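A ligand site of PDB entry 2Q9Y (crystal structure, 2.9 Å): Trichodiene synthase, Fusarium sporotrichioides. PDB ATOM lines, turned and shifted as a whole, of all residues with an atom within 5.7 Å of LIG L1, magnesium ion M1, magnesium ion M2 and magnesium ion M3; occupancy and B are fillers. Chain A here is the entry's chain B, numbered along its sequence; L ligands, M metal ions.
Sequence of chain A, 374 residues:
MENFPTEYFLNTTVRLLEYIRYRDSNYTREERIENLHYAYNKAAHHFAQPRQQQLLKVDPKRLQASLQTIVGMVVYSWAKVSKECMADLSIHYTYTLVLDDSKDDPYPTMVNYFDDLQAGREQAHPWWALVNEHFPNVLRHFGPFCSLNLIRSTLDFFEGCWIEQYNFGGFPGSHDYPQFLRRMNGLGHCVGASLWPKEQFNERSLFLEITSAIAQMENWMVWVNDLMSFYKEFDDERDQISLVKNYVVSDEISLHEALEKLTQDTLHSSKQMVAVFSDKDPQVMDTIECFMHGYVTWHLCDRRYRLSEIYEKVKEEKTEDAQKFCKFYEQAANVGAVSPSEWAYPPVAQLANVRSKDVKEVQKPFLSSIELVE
An oxygen (O7) of LIG L1 is in hydrogen-bond range of the side-chain hydroxyl (OH) of Tyr 305, at 2.5 Å. An oxygen (O5) of LIG L1 sits close to the side-chain carboxylate (OE2) of Glu 233 (2.8 Å). NH1 of Arg 182 is in salt-bridge range of O3 of LIG L1, 2.7 Å away. The side-chain hydroxyl (OG) of Ser 229 sits at hydrogen-bond distance from an oxygen (O5) of LIG L1, 3.1 Å away. An oxygen (O7) of LIG L1 is in salt-bridge range of the guanidinium group (NE) of Arg 304 (3.3 Å). The side-chain amino group (NZ) of Lys 232 lies close to an oxygen (O6) of LIG L1, 3.2 Å away.
ND2 of Asn 225 is in hydrogen-bond range of OH of Tyr 305 (3.4 Å). NH2 of Arg 182 sits close to OD1 of Asn 225 (3.1 Å). The guanidinium group of Arg 304 is in salt-bridge range of the side-chain carboxylate of Asp 100. The side-chain carboxylate (OE1) of Glu 233 is in hydrogen-bond range of the side-chain hydroxyl (OG) of Ser 229. NE of Arg 182 is in salt-bridge range of OD2 of Asp 226, at 2.9 Å. O of Arg 182 lies close to OD1 of Asn 185 (3.1 Å). The backbone carbonyl oxygen (O) of Val 222 lies within hydrogen-bond range of the guanidinium group (NH2) of Arg 182 (3.1 Å). The guanidinium group (NH1) of Arg 304 is in salt-bridge range of the side-chain carboxylate (OD2) of Asp 101 (3.1 Å).
Eight residues have an atom within 4 Å of LIG L1: Asp 100, Arg 182, Asn 225, Ser 229, Lys 232, Glu 233, Arg 304 and Tyr 305. The nearest printed residue that does not touch LIG L1 is Asn 185 (4.1 Å).
Arg 182 touches magnesium ion M1. Asp 226 touches magnesium ion M1 (OD1 to MG, 3.8 Å). Along chain A the residues within 4 Å of magnesium ion M1 span positions 182 to 233.
Residues that only touch magnesium ion M2: Arg 304 and Lys 232. Of the 21 residues printed, 3 come within 4 Å of magnesium ion M2.
Merely in contact with magnesium ion M3: Glu 164. Two residues have an atom within 4 Å of magnesium ion M3: Asp 100 and Glu 164. The nearest printed residue that does not touch magnesium ion M3 is Asn 185 (4.2 Å).
Magnesium ion M1 is bound by OD1 of Asn 225 (2.3 Å) and O1 of LIG L1 (2.5 Å). Slightly farther from magnesium ion M1 lies the side-chain carboxylate (OE1) of Glu 233 (2.6 Å). Slightly farther from magnesium ion M1 lies an oxygen (O5) of LIG L1 (2.7 Å). Slightly farther from magnesium ion M1 lies the side-chain hydroxyl (OG) of Ser 229 (2.7 Å). Slightly farther from magnesium ion M1 lies the side-chain carboxylate (OE2) of Glu 233 (2.8 Å).
Magnesium ion M2 is bound by an oxygen (O6) of LIG L1. Magnesium ion M2 has one donor atom within binding distance. Slightly farther from magnesium ion M2 lies an oxygen (O2) of LIG L1 (2.7 Å).
Magnesium ion M3 is bound by an oxygen (O2) of LIG L1 (2.2 Å) and the side-chain carboxylate of Asp 100 (2.3 Å). Slightly farther from magnesium ion M3 lies OD1 of Asp 100 (2.7 Å).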
ATOM      1  N   LEU A  97       6.763   5.843 -32.709  1.00  0.00           N
ATOM      2  CA  LEU A  97       7.410   4.646 -32.180  1.00  0.00           C
ATOM      3  C   LEU A  97       8.869   4.894 -31.848  1.00  0.00           C
ATOM      4  O   LEU A  97       9.419   4.275 -30.945  1.00  0.00           O
ATOM      5  CB  LEU A  97       7.312   3.486 -33.182  1.00  0.00           C
ATOM      6  CG  LEU A  97       7.804   2.156 -32.584  1.00  0.00           C
ATOM      7  CD1 LEU A  97       7.093   1.959 -31.264  1.00  0.00           C
ATOM      8  CD2 LEU A  97       7.547   0.982 -33.538  1.00  0.00           C
ATOM      9  N   ASP A 100       8.725   6.590 -28.482  1.00  0.00           N
ATOM     10  CA  ASP A 100       8.264   5.639 -27.462  1.00  0.00           C
ATOM     11  C   ASP A 100       9.401   4.807 -26.886  1.00  0.00           C
ATOM     12  O   ASP A 100       9.377   4.430 -25.719  1.00  0.00           O
ATOM     13  CB  ASP A 100       7.209   4.696 -28.045  1.00  0.00           C
ATOM     14  CG  ASP A 100       6.632   3.730 -27.010  1.00  0.00           C
ATOM     15  OD1 ASP A 100       5.954   2.758 -27.410  1.00  0.00           O
ATOM     16  OD2 ASP A 100       6.839   3.951 -25.792  1.00  0.00           O
ATOM     17  N   ASP A 101      10.388   4.517 -27.720  1.00  0.00           N
ATOM     18  CA  ASP A 101      11.515   3.706 -27.287  1.00  0.00           C
ATOM     19  C   ASP A 101      12.756   4.517 -26.957  1.00  0.00           C
ATOM     20  O   ASP A 101      13.793   3.950 -26.627  1.00  0.00           O
ATOM     21  CB  ASP A 101      11.879   2.660 -28.344  1.00  0.00           C
ATOM     22  CG  ASP A 101      10.828   1.561 -28.478  1.00  0.00           C
ATOM     23  OD1 ASP A 101      10.316   1.082 -27.436  1.00  0.00           O
ATOM     24  OD2 ASP A 101      10.545   1.162 -29.635  1.00  0.00           O
ATOM     25  N   PHE A 157       0.473  12.054 -26.161  1.00  0.00           N
ATOM     26  CA  PHE A 157       1.443  10.983 -26.269  1.00  0.00           C
ATOM     27  C   PHE A 157       2.854  11.525 -26.027  1.00  0.00           C
ATOM     28  O   PHE A 157       3.708  10.844 -25.478  1.00  0.00           O
ATOM     29  CB  PHE A 157       1.352  10.365 -27.660  1.00  0.00           C
ATOM     30  CG  PHE A 157       2.465   9.416 -27.976  1.00  0.00           C
ATOM     31  CD1 PHE A 157       2.516   8.176 -27.364  1.00  0.00           C
ATOM     32  CD2 PHE A 157       3.486   9.798 -28.832  1.00  0.00           C
ATOM     33  CE1 PHE A 157       3.571   7.326 -27.608  1.00  0.00           C
ATOM     34  CE2 PHE A 157       4.550   8.942 -29.086  1.00  0.00           C
ATOM     35  CZ  PHE A 157       4.593   7.708 -28.464  1.00  0.00           C
ATOM     36  N   CYS A 161       5.384  10.092 -22.935  1.00  0.00           N
ATOM     37  CA  CYS A 161       6.761   9.617 -23.097  1.00  0.00           C
ATOM     38  C   CYS A 161       7.701  10.355 -22.158  1.00  0.00           C
ATOM     39  O   CYS A 161       8.656   9.781 -21.633  1.00  0.00           O
ATOM     40  CB  CYS A 161       7.220   9.807 -24.550  1.00  0.00           C
ATOM     41  SG  CYS A 161       6.490   8.634 -25.722  1.00  0.00           S
ATOM     42  N   GLU A 164       7.108   9.203 -18.698  1.00  0.00           N
ATOM     43  CA  GLU A 164       7.714   7.868 -18.646  1.00  0.00           C
ATOM     44  C   GLU A 164       9.230   7.863 -18.410  1.00  0.00           C
ATOM     45  O   GLU A 164       9.773   6.882 -17.901  1.00  0.00           O
ATOM     46  CB  GLU A 164       7.439   7.099 -19.945  1.00  0.00           C
ATOM     47  CG  GLU A 164       6.016   6.582 -20.109  1.00  0.00           C
ATOM     48  CD  GLU A 164       5.918   5.571 -21.237  1.00  0.00           C
ATOM     49  OE1 GLU A 164       6.189   5.940 -22.411  1.00  0.00           O
ATOM     50  OE2 GLU A 164       5.573   4.408 -20.943  1.00  0.00           O
ATOM     51  N   ARG A 182      -1.493   5.627 -18.714  1.00  0.00           N
ATOM     52  CA  ARG A 182      -1.727   4.779 -19.885  1.00  0.00           C
ATOM     53  C   ARG A 182      -2.505   5.495 -20.983  1.00  0.00           C
ATOM     54  O   ARG A 182      -2.221   5.331 -22.171  1.00  0.00           O
ATOM     55  CB  ARG A 182      -2.470   3.503 -19.486  1.00  0.00           C
ATOM     56  CG  ARG A 182      -2.661   2.528 -20.655  1.00  0.00           C
ATOM     57  CD  ARG A 182      -1.434   2.445 -21.549  1.00  0.00           C
ATOM     58  NE  ARG A 182      -1.554   1.336 -22.484  1.00  0.00           N
ATOM     59  CZ  ARG A 182      -0.774   1.142 -23.534  1.00  0.00           C
ATOM     60  NH1 ARG A 182       0.210   1.992 -23.804  1.00  0.00           N
ATOM     61  NH2 ARG A 182      -0.969   0.093 -24.323  1.00  0.00           N
ATOM     62  N   ASN A 185      -0.347   7.949 -23.057  1.00  0.00           N
ATOM     63  CA  ASN A 185       0.623   7.464 -24.032  1.00  0.00           C
ATOM     64  C   ASN A 185       0.110   6.400 -24.980  1.00  0.00           C
ATOM     65  O   ASN A 185       0.879   5.856 -25.791  1.00  0.00           O
ATOM     66  CB  ASN A 185       1.865   6.932 -23.319  1.00  0.00           C
ATOM     67  CG  ASN A 185       1.531   5.872 -22.292  1.00  0.00           C
ATOM     68  OD1 ASN A 185       0.789   4.909 -22.570  1.00  0.00           O
ATOM     69  ND2 ASN A 185       2.081   6.032 -21.088  1.00  0.00           N
ATOM     70  N   GLY A 186      -1.192   6.101 -24.899  1.00  0.00           N
ATOM     71  CA  GLY A 186      -1.769   5.096 -25.762  1.00  0.00           C
ATOM     72  C   GLY A 186      -2.258   5.536 -27.131  1.00  0.00           C
ATOM     73  O   GLY A 186      -2.814   4.712 -27.872  1.00  0.00           O
ATOM     74  N   VAL A 222      -5.814  -0.024 -26.306  1.00  0.00           N
ATOM     75  CA  VAL A 222      -4.695  -0.017 -25.365  1.00  0.00           C
ATOM     76  C   VAL A 222      -4.575  -1.215 -24.427  1.00  0.00           C
ATOM     77  O   VAL A 222      -3.458  -1.670 -24.162  1.00  0.00           O
ATOM     78  CB  VAL A 222      -4.708   1.259 -24.513  1.00  0.00           C
ATOM     79  CG1 VAL A 222      -4.486   2.471 -25.392  1.00  0.00           C
ATOM     80  CG2 VAL A 222      -6.019   1.371 -23.761  1.00  0.00           C
ATOM     81  N   ASN A 225      -3.203  -4.257 -26.070  1.00  0.00           N
ATOM     82  CA  ASN A 225      -1.760  -4.188 -26.201  1.00  0.00           C
ATOM     83  C   ASN A 225      -1.118  -4.422 -24.848  1.00  0.00           C
ATOM     84  O   ASN A 225      -0.092  -5.098 -24.738  1.00  0.00           O
ATOM     85  CB  ASN A 225      -1.309  -2.838 -26.750  1.00  0.00           C
ATOM     86  CG  ASN A 225       0.190  -2.629 -26.606  1.00  0.00           C
ATOM     87  OD1 ASN A 225       0.678  -2.261 -25.533  1.00  0.00           O
ATOM     88  ND2 ASN A 225       0.927  -2.873 -27.679  1.00  0.00           N
ATOM     89  N   ASP A 226      -1.718  -3.856 -23.803  1.00  0.00           N
ATOM     90  CA  ASP A 226      -1.170  -4.030 -22.463  1.00  0.00           C
ATOM     91  C   ASP A 226      -1.075  -5.509 -22.149  1.00  0.00           C
ATOM     92  O   ASP A 226      -0.196  -5.949 -21.405  1.00  0.00           O
ATOM     93  CB  ASP A 226      -2.066  -3.340 -21.432  1.00  0.00           C
ATOM     94  CG  ASP A 226      -1.749  -1.873 -21.295  1.00  0.00           C
ATOM     95  OD1 ASP A 226      -0.553  -1.533 -21.136  1.00  0.00           O
ATOM     96  OD2 ASP A 226      -2.696  -1.060 -21.342  1.00  0.00           O
ATOM     97  N   SER A 229       1.360  -7.633 -25.229  1.00  0.00           N
ATOM     98  CA  SER A 229       2.771  -7.299 -25.086  1.00  0.00           C
ATOM     99  C   SER A 229       3.268  -7.384 -23.643  1.00  0.00           C
ATOM    100  O   SER A 229       4.343  -6.863 -23.318  1.00  0.00           O
ATOM    101  CB  SER A 229       3.052  -5.888 -25.645  1.00  0.00           C
ATOM    102  OG  SER A 229       2.464  -4.867 -24.860  1.00  0.00           O
ATOM    103  N   LYS A 232       6.921  -9.207 -23.954  1.00  0.00           N
ATOM    104  CA  LYS A 232       8.072  -8.401 -24.366  1.00  0.00           C
ATOM    105  C   LYS A 232       8.408  -7.221 -23.444  1.00  0.00           C
ATOM    106  O   LYS A 232       9.551  -6.753 -23.408  1.00  0.00           O
ATOM    107  CB  LYS A 232       7.850  -7.898 -25.811  1.00  0.00           C
ATOM    108  CG  LYS A 232       6.994  -6.645 -25.977  1.00  0.00           C
ATOM    109  CD  LYS A 232       7.851  -5.367 -25.947  1.00  0.00           C
ATOM    110  CE  LYS A 232       7.034  -4.101 -26.227  1.00  0.00           C
ATOM    111  NZ  LYS A 232       7.855  -2.857 -26.161  1.00  0.00           N
ATOM    112  N   GLU A 233       7.420  -6.733 -22.691  1.00  0.00           N
ATOM    113  CA  GLU A 233       7.633  -5.612 -21.780  1.00  0.00           C
ATOM    114  C   GLU A 233       7.964  -6.089 -20.371  1.00  0.00           C
ATOM    115  O   GLU A 233       8.000  -5.282 -19.431  1.00  0.00           O
ATOM    116  CB  GLU A 233       6.378  -4.727 -21.694  1.00  0.00           C
ATOM    117  CG  GLU A 233       5.907  -4.113 -23.002  1.00  0.00           C
ATOM    118  CD  GLU A 233       4.738  -3.175 -22.794  1.00  0.00           C
ATOM    119  OE1 GLU A 233       3.737  -3.591 -22.156  1.00  0.00           O
ATOM    120  OE2 GLU A 233       4.813  -2.016 -23.260  1.00  0.00           O
ATOM    121  N   ARG A 238      12.604   0.718 -19.691  1.00  0.00           N
ATOM    122  CA  ARG A 238      11.754   1.658 -20.448  1.00  0.00           C
ATOM    123  C   ARG A 238      10.351   1.063 -20.544  1.00  0.00           C
ATOM    124  O   ARG A 238       9.342   1.788 -20.459  1.00  0.00           O
ATOM    125  CB  ARG A 238      12.326   1.936 -21.853  1.00  0.00           C
ATOM    126  CG  ARG A 238      11.282   2.229 -22.959  1.00  0.00           C
ATOM    127  CD  ARG A 238      10.330   3.400 -22.681  1.00  0.00           C
ATOM    128  NE  ARG A 238      10.934   4.714 -22.889  1.00  0.00           N
ATOM    129  CZ  ARG A 238      10.234   5.854 -22.897  1.00  0.00           C
ATOM    130  NH1 ARG A 238       8.924   5.820 -22.723  1.00  0.00           N
ATOM    131  NH2 ARG A 238      10.858   7.010 -23.078  1.00  0.00           N
ATOM    132  N   ASP A 239      10.288  -0.243 -20.726  1.00  0.00           N
ATOM    133  CA  ASP A 239       9.010  -0.951 -20.774  1.00  0.00           C
ATOM    134  C   ASP A 239       8.775  -1.379 -19.323  1.00  0.00           C
ATOM    135  O   ASP A 239       7.792  -2.047 -18.992  1.00  0.00           O
ATOM    136  CB  ASP A 239       9.044  -2.034 -21.858  1.00  0.00           C
ATOM    137  N   SER A 242       4.689  -0.099 -16.940  1.00  0.00           N
ATOM    138  CA  SER A 242       3.506  -0.454 -17.731  1.00  0.00           C
ATOM    139  C   SER A 242       2.252  -0.462 -16.867  1.00  0.00           C
ATOM    140  O   SER A 242       2.321  -0.566 -15.651  1.00  0.00           O
ATOM    141  CB  SER A 242       3.703  -1.829 -18.387  1.00  0.00           C
ATOM    142  OG  SER A 242       3.899  -2.847 -17.411  1.00  0.00           O
ATOM    143  N   TRP A 298      -1.528  -8.786 -36.035  1.00  0.00           N
ATOM    144  CA  TRP A 298      -0.240  -8.106 -35.995  1.00  0.00           C
ATOM    145  C   TRP A 298       0.529  -8.402 -34.710  1.00  0.00           C
ATOM    146  O   TRP A 298       1.756  -8.555 -34.731  1.00  0.00           O
ATOM    147  CB  TRP A 298      -0.461  -6.609 -36.156  1.00  0.00           C
ATOM    148  CG  TRP A 298       0.756  -5.733 -36.014  1.00  0.00           C
ATOM    149  CD1 TRP A 298       1.822  -5.632 -36.862  1.00  0.00           C
ATOM    150  CD2 TRP A 298       0.975  -4.774 -34.975  1.00  0.00           C
ATOM    151  NE1 TRP A 298       2.689  -4.649 -36.429  1.00  0.00           N
ATOM    152  CE2 TRP A 298       2.184  -4.110 -35.263  1.00  0.00           C
ATOM    153  CE3 TRP A 298       0.259  -4.399 -33.826  1.00  0.00           C
ATOM    154  CZ2 TRP A 298       2.701  -3.096 -34.450  1.00  0.00           C
ATOM    155  CZ3 TRP A 298       0.762  -3.392 -33.022  1.00  0.00           C
ATOM    156  CH2 TRP A 298       1.972  -2.753 -33.337  1.00  0.00           C
ATOM    157  N   ARG A 304       8.609  -7.369 -32.740  1.00  0.00           N
ATOM    158  CA  ARG A 304       8.541  -6.542 -31.538  1.00  0.00           C
ATOM    159  C   ARG A 304       7.901  -7.241 -30.328  1.00  0.00           C
ATOM    160  O   ARG A 304       8.436  -7.196 -29.222  1.00  0.00           O
ATOM    161  CB  ARG A 304       7.776  -5.257 -31.841  1.00  0.00           C
ATOM    162  CG  ARG A 304       7.833  -4.240 -30.713  1.00  0.00           C
ATOM    163  CD  ARG A 304       6.748  -3.191 -30.841  1.00  0.00           C
ATOM    164  NE  ARG A 304       6.827  -2.201 -29.771  1.00  0.00           N
ATOM    165  CZ  ARG A 304       7.795  -1.298 -29.644  1.00  0.00           C
ATOM    166  NH1 ARG A 304       8.778  -1.265 -30.542  1.00  0.00           N
ATOM    167  NH2 ARG A 304       7.785  -0.442 -28.637  1.00  0.00           N
ATOM    168  N   TYR A 305       6.752  -7.882 -30.547  1.00  0.00           N
ATOM    169  CA  TYR A 305       6.057  -8.561 -29.459  1.00  0.00           C
ATOM    170  C   TYR A 305       6.490  -9.992 -29.271  1.00  0.00           C
ATOM    171  O   TYR A 305       5.991 -10.702 -28.386  1.00  0.00           O
ATOM    172  CB  TYR A 305       4.551  -8.482 -29.683  1.00  0.00           C
ATOM    173  CG  TYR A 305       4.113  -7.060 -29.779  1.00  0.00           C
ATOM    174  CD1 TYR A 305       4.354  -6.175 -28.733  1.00  0.00           C
ATOM    175  CD2 TYR A 305       3.538  -6.560 -30.951  1.00  0.00           C
ATOM    176  CE1 TYR A 305       4.049  -4.823 -28.846  1.00  0.00           C
ATOM    177  CE2 TYR A 305       3.224  -5.205 -31.074  1.00  0.00           C
ATOM    178  CZ  TYR A 305       3.485  -4.349 -30.016  1.00  0.00           C
ATOM    179  OH  TYR A 305       3.221  -3.004 -30.130  1.00  0.00           O
HETATM  180  P1  LIG L   1       3.105   1.006 -25.318  1.00  0.00           P
HETATM  181  O1  LIG L   1       2.518   0.041 -24.313  1.00  0.00           O
HETATM  182  O2  LIG L   1       4.315   1.725 -24.766  1.00  0.00           O
HETATM  183  O3  LIG L   1       2.094   1.989 -25.732  1.00  0.00           O
HETATM  184  O4  LIG L   1       3.259   0.147 -26.660  1.00  0.00           O
HETATM  185  P2  LIG L   1       4.267  -1.146 -26.836  1.00  0.00           P
HETATM  186  O5  LIG L   1       3.846  -2.283 -25.858  1.00  0.00           O
HETATM  187  O6  LIG L   1       5.658  -0.622 -26.551  1.00  0.00           O
HETATM  188  O7  LIG L   1       4.010  -1.517 -28.218  1.00  0.00           O
HETATM  189  N1  LG2 L   2      -0.345   1.306 -29.651  1.00  0.00           N
HETATM  190  C1  LG2 L   2       1.082   1.692 -29.111  1.00  0.00           C
HETATM  191  C2  LG2 L   2      -1.118   2.564 -30.212  1.00  0.00           C
HETATM  192  C3  LG2 L   2      -0.910   2.977 -31.701  1.00  0.00           C
HETATM  193  C4  LG2 L   2      -1.184   0.777 -28.463  1.00  0.00           C
HETATM  194  C5  LG2 L   2      -1.428   1.703 -27.245  1.00  0.00           C
HETATM  195  C6  LG2 L   2      -0.347   0.216 -30.743  1.00  0.00           C
HETATM  196  C7  LG2 L   2       0.354  -1.117 -30.422  1.00  0.00           C
HETATM  197  C8  LG2 L   2       2.150   2.309 -30.023  1.00  0.00           C
HETATM  198  C9  LG2 L   2       2.783   3.531 -29.618  1.00  0.00           C
HETATM  199  C10 LG2 L   2       3.765   4.154 -30.428  1.00  0.00           C
HETATM  200  C11 LG2 L   2       4.144   3.573 -31.656  1.00  0.00           C
HETATM  201  C12 LG2 L   2       3.538   2.360 -32.083  1.00  0.00           C
HETATM  202  C13 LG2 L   2       2.555   1.737 -31.273  1.00  0.00           C
HETATM  203 MG    MG M   1       2.107  -2.368 -23.785  1.00  0.00          MG
HETATM  204 MG    MG M   2       6.839   0.894 -25.379  1.00  0.00          MG
HETATM  205 MG    MG M   3       4.553   3.853 -25.330  1.00  0.00          MG
